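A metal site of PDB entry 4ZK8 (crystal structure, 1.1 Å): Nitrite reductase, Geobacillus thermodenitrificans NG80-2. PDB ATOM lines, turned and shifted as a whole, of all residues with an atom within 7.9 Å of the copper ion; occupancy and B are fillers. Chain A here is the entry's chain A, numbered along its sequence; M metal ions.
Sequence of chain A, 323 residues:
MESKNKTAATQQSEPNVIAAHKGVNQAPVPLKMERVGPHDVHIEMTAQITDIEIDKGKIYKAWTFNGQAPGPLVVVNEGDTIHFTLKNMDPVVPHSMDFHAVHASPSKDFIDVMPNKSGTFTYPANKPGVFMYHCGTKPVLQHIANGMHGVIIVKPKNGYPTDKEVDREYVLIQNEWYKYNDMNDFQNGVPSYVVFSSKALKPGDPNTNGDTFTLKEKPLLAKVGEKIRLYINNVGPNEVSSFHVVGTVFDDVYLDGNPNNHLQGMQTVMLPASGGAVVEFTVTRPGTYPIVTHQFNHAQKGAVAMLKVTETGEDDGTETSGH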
ATOM      1  N   ALA A  47      12.286  29.670  -9.265  1.00  0.00           N
ATOM      2  CA  ALA A  47      12.780  28.788 -10.317  1.00  0.00           C
ATOM      3  C   ALA A  47      14.318  28.879 -10.207  1.00  0.00           C
ATOM      4  O   ALA A  47      14.862  30.005 -10.216  1.00  0.00           O
ATOM      5  CB  ALA A  47      12.334  29.274 -11.695  1.00  0.00           C
ATOM      6  N   ILE A  49      18.321  26.560 -10.719  1.00  0.00           N
ATOM      7  CA  ILE A  49      19.094  25.511 -11.430  1.00  0.00           C
ATOM      8  C   ILE A  49      19.932  24.826 -10.384  1.00  0.00           C
ATOM      9  O   ILE A  49      20.826  25.480  -9.760  1.00  0.00           O
ATOM     10  CB  ILE A  49      19.973  26.172 -12.520  1.00  0.00           C
ATOM     11  CG1 ILE A  49      19.129  26.910 -13.505  1.00  0.00           C
ATOM     12  CG2 ILE A  49      20.853  25.103 -13.209  1.00  0.00           C
ATOM     13  CD1 ILE A  49      17.957  26.126 -14.199  1.00  0.00           C
ATOM     14  N   TRP A  63      16.354  21.813 -13.826  1.00  0.00           N
ATOM     15  CA  TRP A  63      15.522  23.023 -13.746  1.00  0.00           C
ATOM     16  C   TRP A  63      14.508  22.752 -12.738  1.00  0.00           C
ATOM     17  O   TRP A  63      13.786  21.741 -12.871  1.00  0.00           O
ATOM     18  CB  TRP A  63      14.966  23.336 -15.129  1.00  0.00           C
ATOM     19  CG  TRP A  63      15.903  23.523 -16.268  1.00  0.00           C
ATOM     20  CD1 TRP A  63      17.212  23.384 -16.288  1.00  0.00           C
ATOM     21  CD2 TRP A  63      15.534  23.997 -17.580  1.00  0.00           C
ATOM     22  NE1 TRP A  63      17.712  23.691 -17.564  1.00  0.00           N
ATOM     23  CE2 TRP A  63      16.663  24.033 -18.346  1.00  0.00           C
ATOM     24  CE3 TRP A  63      14.279  24.275 -18.139  1.00  0.00           C
ATOM     25  CZ2 TRP A  63      16.653  24.469 -19.670  1.00  0.00           C
ATOM     26  CZ3 TRP A  63      14.274  24.671 -19.505  1.00  0.00           C
ATOM     27  CH2 TRP A  63      15.420  24.730 -20.229  1.00  0.00           C
ATOM     28  N   THR A  64      14.380  23.584 -11.723  1.00  0.00           N
ATOM     29  CA  THR A  64      13.606  23.235 -10.556  1.00  0.00           C
ATOM     30  C   THR A  64      12.756  24.402 -10.016  1.00  0.00           C
ATOM     31  O   THR A  64      13.108  25.574 -10.310  1.00  0.00           O
ATOM     32  CB  THR A  64      14.461  22.802  -9.361  1.00  0.00           C
ATOM     33  OG1 THR A  64      15.129  23.889  -8.764  1.00  0.00           O
ATOM     34  CG2 THR A  64      15.484  21.728  -9.771  1.00  0.00           C
ATOM     35  N   PHE A  65      11.777  24.057  -9.225  1.00  0.00           N
ATOM     36  CA  PHE A  65      11.211  24.937  -8.230  1.00  0.00           C
ATOM     37  C   PHE A  65      11.932  24.717  -6.913  1.00  0.00           C
ATOM     38  O   PHE A  65      11.942  23.600  -6.411  1.00  0.00           O
ATOM     39  CB  PHE A  65       9.749  24.714  -8.094  1.00  0.00           C
ATOM     40  CG  PHE A  65       8.991  25.014  -9.384  1.00  0.00           C
ATOM     41  CD1 PHE A  65       8.739  26.342  -9.765  1.00  0.00           C
ATOM     42  CD2 PHE A  65       8.486  23.980 -10.179  1.00  0.00           C
ATOM     43  CE1 PHE A  65       7.997  26.618 -10.934  1.00  0.00           C
ATOM     44  CE2 PHE A  65       7.746  24.297 -11.311  1.00  0.00           C
ATOM     45  CZ  PHE A  65       7.506  25.603 -11.709  1.00  0.00           C
ATOM     46  N   LEU A  86       6.443  33.794  -8.135  1.00  0.00           N
ATOM     47  CA  LEU A  86       7.583  33.106  -8.643  1.00  0.00           C
ATOM     48  C   LEU A  86       8.759  34.052  -8.797  1.00  0.00           C
ATOM     49  O   LEU A  86       8.637  35.061  -9.537  1.00  0.00           O
ATOM     50  CB  LEU A  86       7.298  32.413 -10.019  1.00  0.00           C
ATOM     51  CG  LEU A  86       8.444  31.565 -10.594  1.00  0.00           C
ATOM     52  CD1 LEU A  86       8.730  30.338  -9.725  1.00  0.00           C
ATOM     53  CD2 LEU A  86       8.104  31.167 -12.014  1.00  0.00           C
ATOM     54  N   ASN A  88      12.326  34.163 -10.369  1.00  0.00           N
ATOM     55  CA  ASN A  88      13.105  33.385 -11.301  1.00  0.00           C
ATOM     56  C   ASN A  88      14.602  33.696 -11.094  1.00  0.00           C
ATOM     57  O   ASN A  88      15.058  34.805 -11.369  1.00  0.00           O
ATOM     58  CB  ASN A  88      12.697  33.730 -12.756  1.00  0.00           C
ATOM     59  CG  ASN A  88      13.399  32.834 -13.722  1.00  0.00           C
ATOM     60  OD1 ASN A  88      14.186  31.975 -13.314  1.00  0.00           O
ATOM     61  ND2 ASN A  88      13.195  33.066 -14.993  1.00  0.00           N
ATOM     62  N   ASP A  90      16.970  31.693 -12.484  1.00  0.00           N
ATOM     63  CA  ASP A  90      17.698  31.213 -13.638  1.00  0.00           C
ATOM     64  C   ASP A  90      18.274  32.446 -14.369  1.00  0.00           C
ATOM     65  O   ASP A  90      17.567  33.415 -14.627  1.00  0.00           O
ATOM     66  CB  ASP A  90      16.715  30.481 -14.579  1.00  0.00           C
ATOM     67  CG  ASP A  90      17.371  29.736 -15.706  1.00  0.00           C
ATOM     68  OD1 ASP A  90      18.363  30.292 -16.351  1.00  0.00           O
ATOM     69  OD2 ASP A  90      16.870  28.652 -16.081  1.00  0.00           O
ATOM     70  N   VAL A  93      16.972  31.595 -18.658  1.00  0.00           N
ATOM     71  CA  VAL A  93      15.713  31.031 -19.192  1.00  0.00           C
ATOM     72  C   VAL A  93      14.552  31.561 -18.422  1.00  0.00           C
ATOM     73  O   VAL A  93      14.547  31.510 -17.180  1.00  0.00           O
ATOM     74  CB  VAL A  93      15.743  29.493 -19.154  1.00  0.00           C
ATOM     75  CG1 VAL A  93      14.578  28.875 -19.889  1.00  0.00           C
ATOM     76  CG2 VAL A  93      16.994  28.908 -19.667  1.00  0.00           C
ATOM     77  N   PRO A  94      13.470  32.014 -19.101  1.00  0.00           N
ATOM     78  CA  PRO A  94      12.236  32.373 -18.426  1.00  0.00           C
ATOM     79  C   PRO A  94      11.535  31.099 -17.849  1.00  0.00           C
ATOM     80  O   PRO A  94      11.733  30.010 -18.413  1.00  0.00           O
ATOM     81  CB  PRO A  94      11.348  33.001 -19.507  1.00  0.00           C
ATOM     82  CG  PRO A  94      12.290  33.365 -20.617  1.00  0.00           C
ATOM     83  CD  PRO A  94      13.393  32.274 -20.566  1.00  0.00           C
ATOM     84  N   HIS A  95      10.744  31.288 -16.820  1.00  0.00           N
ATOM     85  CA  HIS A  95       9.966  30.186 -16.231  1.00  0.00           C
ATOM     86  C   HIS A  95       8.631  30.702 -15.825  1.00  0.00           C
ATOM     87  O   HIS A  95       8.347  31.930 -15.726  1.00  0.00           O
ATOM     88  CB  HIS A  95      10.711  29.530 -15.038  1.00  0.00           C
ATOM     89  CG  HIS A  95      11.999  28.926 -15.434  1.00  0.00           C
ATOM     90  ND1 HIS A  95      12.094  27.766 -16.170  1.00  0.00           N
ATOM     91  CD2 HIS A  95      13.264  29.316 -15.188  1.00  0.00           C
ATOM     92  CE1 HIS A  95      13.344  27.519 -16.403  1.00  0.00           C
ATOM     93  NE2 HIS A  95      14.086  28.421 -15.818  1.00  0.00           N
ATOM     94  N   SER A  96       7.713  29.788 -15.493  1.00  0.00           N
ATOM     95  CA  SER A  96       6.338  30.080 -15.200  1.00  0.00           C
ATOM     96  C   SER A  96       5.755  29.033 -14.239  1.00  0.00           C
ATOM     97  O   SER A  96       6.482  28.018 -13.966  1.00  0.00           O
ATOM     98  CB  SER A  96       5.497  30.196 -16.471  1.00  0.00           C
ATOM     99  OG  SER A  96       5.569  28.982 -17.200  1.00  0.00           O
ATOM    100  N   MET A  97       4.517  29.178 -13.884  1.00  0.00           N
ATOM    101  CA  MET A  97       3.872  28.188 -13.044  1.00  0.00           C
ATOM    102  C   MET A  97       2.449  27.951 -13.515  1.00  0.00           C
ATOM    103  O   MET A  97       1.635  28.895 -13.659  1.00  0.00           O
ATOM    104  CB  MET A  97       3.801  28.671 -11.589  1.00  0.00           C
ATOM    105  CG  MET A  97       3.038  27.773 -10.646  1.00  0.00           C
ATOM    106  SD  MET A  97       3.625  26.075 -10.501  1.00  0.00           S
ATOM    107  CE  MET A  97       4.871  26.332  -9.268  1.00  0.00           C
ATOM    108  N   ASP A 112       5.203  33.888 -18.405  1.00  0.00           N
ATOM    109  CA  ASP A 112       6.617  33.872 -18.071  1.00  0.00           C
ATOM    110  C   ASP A 112       7.044  34.969 -17.126  1.00  0.00           C
ATOM    111  O   ASP A 112       6.611  36.112 -17.232  1.00  0.00           O
ATOM    112  CB  ASP A 112       7.443  33.894 -19.347  1.00  0.00           C
ATOM    113  CG  ASP A 112       7.292  32.613 -20.212  1.00  0.00           C
ATOM    114  OD1 ASP A 112       6.822  31.570 -19.726  1.00  0.00           O
ATOM    115  OD2 ASP A 112       7.645  32.637 -21.391  1.00  0.00           O
ATOM    116  N   VAL A 113       8.011  34.612 -16.303  1.00  0.00           N
ATOM    117  CA  VAL A 113       8.794  35.512 -15.432  1.00  0.00           C
ATOM    118  C   VAL A 113      10.169  35.446 -15.914  1.00  0.00           C
ATOM    119  O   VAL A 113      10.789  34.340 -16.040  1.00  0.00           O
ATOM    120  CB  VAL A 113       8.642  35.071 -13.990  1.00  0.00           C
ATOM    121  CG1 VAL A 113       9.504  35.961 -13.087  1.00  0.00           C
ATOM    122  CG2 VAL A 113       7.221  35.017 -13.546  1.00  0.00           C
ATOM    123  N   HIS A 134       3.457  22.516 -12.592  1.00  0.00           N
ATOM    124  CA  HIS A 134       4.637  22.466 -13.436  1.00  0.00           C
ATOM    125  C   HIS A 134       4.884  23.801 -14.097  1.00  0.00           C
ATOM    126  O   HIS A 134       3.981  24.637 -14.182  1.00  0.00           O
ATOM    127  CB  HIS A 134       4.478  21.362 -14.500  1.00  0.00           C
ATOM    128  CG  HIS A 134       3.278  21.543 -15.410  1.00  0.00           C
ATOM    129  ND1 HIS A 134       3.329  22.268 -16.575  1.00  0.00           N
ATOM    130  CD2 HIS A 134       2.028  21.010 -15.356  1.00  0.00           C
ATOM    131  CE1 HIS A 134       2.145  22.200 -17.191  1.00  0.00           C
ATOM    132  NE2 HIS A 134       1.334  21.436 -16.486  1.00  0.00           N
ATOM    133  N   CYS A 135       6.099  23.993 -14.560  1.00  0.00           N
ATOM    134  CA  CYS A 135       6.407  25.121 -15.439  1.00  0.00           C
ATOM    135  C   CYS A 135       5.564  25.044 -16.692  1.00  0.00           C
ATOM    136  O   CYS A 135       5.443  23.961 -17.272  1.00  0.00           O
ATOM    137  CB  CYS A 135       7.864  25.228 -15.645  1.00  0.00           C
ATOM    138  SG  CYS A 135       8.376  26.610 -16.695  1.00  0.00           S
ATOM    139  N   GLY A 136       5.111  26.202 -17.203  1.00  0.00           N
ATOM    140  CA  GLY A 136       4.348  26.282 -18.385  1.00  0.00           C
ATOM    141  C   GLY A 136       4.985  27.042 -19.511  1.00  0.00           C
ATOM    142  O   GLY A 136       4.289  27.553 -20.410  1.00  0.00           O
ATOM    143  N   THR A 137       6.316  27.148 -19.505  1.00  0.00           N
ATOM    144  CA  THR A 137       6.996  27.932 -20.511  1.00  0.00           C
ATOM    145  C   THR A 137       7.303  27.092 -21.692  1.00  0.00           C
ATOM    146  O   THR A 137       7.738  25.928 -21.599  1.00  0.00           O
ATOM    147  CB  THR A 137       8.331  28.459 -19.854  1.00  0.00           C
ATOM    148  OG1 THR A 137       7.931  29.315 -18.764  1.00  0.00           O
ATOM    149  CG2 THR A 137       9.166  29.252 -20.823  1.00  0.00           C
ATOM    150  N   LYS A 138       7.123  27.633 -22.920  1.00  0.00           N
ATOM    151  CA  LYS A 138       7.379  26.915 -24.136  1.00  0.00           C
ATOM    152  C   LYS A 138       8.863  26.652 -24.300  1.00  0.00           C
ATOM    153  O   LYS A 138       9.665  27.618 -24.148  1.00  0.00           O
ATOM    154  CB  LYS A 138       6.864  27.740 -25.342  1.00  0.00           C
ATOM    155  CG  LYS A 138       7.026  27.083 -26.693  1.00  0.00           C
ATOM    156  CD  LYS A 138       6.430  27.919 -27.822  1.00  0.00           C
ATOM    157  CE  LYS A 138       6.239  27.056 -29.036  1.00  0.00           C
ATOM    158  NZ  LYS A 138       5.477  27.810 -30.062  1.00  0.00           N
ATOM    159  N   PRO A 139       9.349  25.468 -24.756  1.00  0.00           N
ATOM    160  CA  PRO A 139       8.550  24.231 -24.912  1.00  0.00           C
ATOM    161  C   PRO A 139       8.246  23.606 -23.557  1.00  0.00           C
ATOM    162  O   PRO A 139       9.222  23.295 -22.801  1.00  0.00           O
ATOM    163  CB  PRO A 139       9.463  23.396 -25.741  1.00  0.00           C
ATOM    164  CG  PRO A 139      10.657  24.150 -26.034  1.00  0.00           C
ATOM    165  CD  PRO A 139      10.720  25.301 -25.105  1.00  0.00           C
ATOM    166  N   VAL A 140       6.993  23.359 -23.279  1.00  0.00           N
ATOM    167  CA  VAL A 140       6.668  22.871 -21.935  1.00  0.00           C
ATOM    168  C   VAL A 140       7.298  21.485 -21.700  1.00  0.00           C
ATOM    169  O   VAL A 140       7.756  21.227 -20.568  1.00  0.00           O
ATOM    170  CB  VAL A 140       5.117  22.826 -21.753  1.00  0.00           C
ATOM    171  CG1 VAL A 140       4.715  22.138 -20.471  1.00  0.00           C
ATOM    172  CG2 VAL A 140       4.585  24.254 -21.783  1.00  0.00           C
ATOM    173  N   GLN A 142      10.197  20.562 -22.483  1.00  0.00           N
ATOM    174  CA  GLN A 142      11.573  20.784 -22.027  1.00  0.00           C
ATOM    175  C   GLN A 142      11.611  21.140 -20.556  1.00  0.00           C
ATOM    176  O   GLN A 142      12.470  20.684 -19.779  1.00  0.00           O
ATOM    177  CB  GLN A 142      12.218  21.856 -22.914  1.00  0.00           C
ATOM    178  CG  GLN A 142      13.688  22.096 -22.573  1.00  0.00           C
ATOM    179  CD  GLN A 142      14.297  23.048 -23.521  1.00  0.00           C
ATOM    180  OE1 GLN A 142      13.636  23.847 -24.210  1.00  0.00           O
ATOM    181  NE2 GLN A 142      15.587  23.061 -23.551  1.00  0.00           N
ATOM    182  N   HIS A 143      10.705  22.075 -20.171  1.00  0.00           N
ATOM    183  CA  HIS A 143      10.708  22.563 -18.804  1.00  0.00           C
ATOM    184  C   HIS A 143      10.287  21.484 -17.848  1.00  0.00           C
ATOM    185  O   HIS A 143      10.901  21.283 -16.756  1.00  0.00           O
ATOM    186  CB  HIS A 143       9.885  23.810 -18.658  1.00  0.00           C
ATOM    187  CG  HIS A 143      10.486  24.994 -19.326  1.00  0.00           C
ATOM    188  ND1 HIS A 143      11.056  26.032 -18.580  1.00  0.00           N
ATOM    189  CD2 HIS A 143      10.681  25.280 -20.649  1.00  0.00           C
ATOM    190  CE1 HIS A 143      11.556  26.895 -19.430  1.00  0.00           C
ATOM    191  NE2 HIS A 143      11.347  26.499 -20.663  1.00  0.00           N
ATOM    192  N   ILE A 144       9.252  20.690 -18.175  1.00  0.00           N
ATOM    193  CA  ILE A 144       8.870  19.592 -17.322  1.00  0.00           C
ATOM    194  C   ILE A 144       9.977  18.544 -17.268  1.00  0.00           C
ATOM    195  O   ILE A 144      10.389  18.079 -16.168  1.00  0.00           O
ATOM    196  CB  ILE A 144       7.522  18.932 -17.762  1.00  0.00           C
ATOM    197  CG1 ILE A 144       6.403  19.966 -17.685  1.00  0.00           C
ATOM    198  CG2 ILE A 144       7.240  17.744 -16.892  1.00  0.00           C
ATOM    199  CD1 ILE A 144       5.042  19.418 -18.194  1.00  0.00           C
ATOM    200  N   ASN A 146      13.090  18.648 -17.655  1.00  0.00           N
ATOM    201  CA  ASN A 146      14.269  19.094 -16.917  1.00  0.00           C
ATOM    202  C   ASN A 146      14.051  19.175 -15.389  1.00  0.00           C
ATOM    203  O   ASN A 146      15.066  19.385 -14.698  1.00  0.00           O
ATOM    204  CB  ASN A 146      14.838  20.367 -17.478  1.00  0.00           C
ATOM    205  CG  ASN A 146      15.633  20.204 -18.709  1.00  0.00           C
ATOM    206  OD1 ASN A 146      16.376  19.170 -18.928  1.00  0.00           O
ATOM    207  ND2 ASN A 146      15.631  21.196 -19.594  1.00  0.00           N
ATOM    208  N   GLY A 147      12.844  19.017 -14.918  1.00  0.00           N
ATOM    209  CA  GLY A 147      12.539  18.881 -13.523  1.00  0.00           C
ATOM    210  C   GLY A 147      11.492  19.804 -12.950  1.00  0.00           C
ATOM    211  O   GLY A 147      11.236  19.697 -11.759  1.00  0.00           O
ATOM    212  N   MET A 148      10.809  20.608 -13.784  1.00  0.00           N
ATOM    213  CA  MET A 148       9.898  21.610 -13.210  1.00  0.00           C
ATOM    214  C   MET A 148       8.477  21.071 -13.108  1.00  0.00           C
ATOM    215  O   MET A 148       7.577  21.424 -13.882  1.00  0.00           O
ATOM    216  CB  MET A 148       9.950  22.879 -14.076  1.00  0.00           C
ATOM    217  CG  MET A 148      11.371  23.417 -14.178  1.00  0.00           C
ATOM    218  SD  MET A 148      11.556  25.110 -14.769  1.00  0.00           S
ATOM    219  CE  MET A 148      11.052  25.961 -13.320  1.00  0.00           C
HETATM  220 CU    CU M   1      10.540  26.548 -16.689  1.00  0.00          CU
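A ring nitrogen (ND1) of His 143 binds the copper ion (2.0 Å). ND1 of His 95 is bound to the copper ion. The side-chain sulfur (SG) of Cys 135 binds the copper ion (2.2 Å). The side-chain sulfur (SD) of Met 148 binds the copper ion (2.6 Å). The copper ion has four donor atoms within binding distance.
Within 4 Å of the copper ion: His 95, Cys 135, His 143 and Met 148. Along chain A the residues within 4 Å of the copper ion span positions 95 to 148.
The side-chain carboxylate of Asp 90 sits at hydrogen-bond distance from a ring nitrogen (NE2) of His 95. The side-chain sulfur of Cys 135 lies close to the backbone NH of Ser 96, 3.5 Å away. O of His 95 sits at hydrogen-bond distance from N of Val 113, 2.8 Å away. O of Trp 63 sits close to N of Met 148 (3.3 Å). The side-chain sulfur (SG) of Cys 135 lies close to the side-chain hydroxyl (OG1) of Thr 137 (3.4 Å). NE2 of His 95 lies close to O of Val 93, 3.4 Å away.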
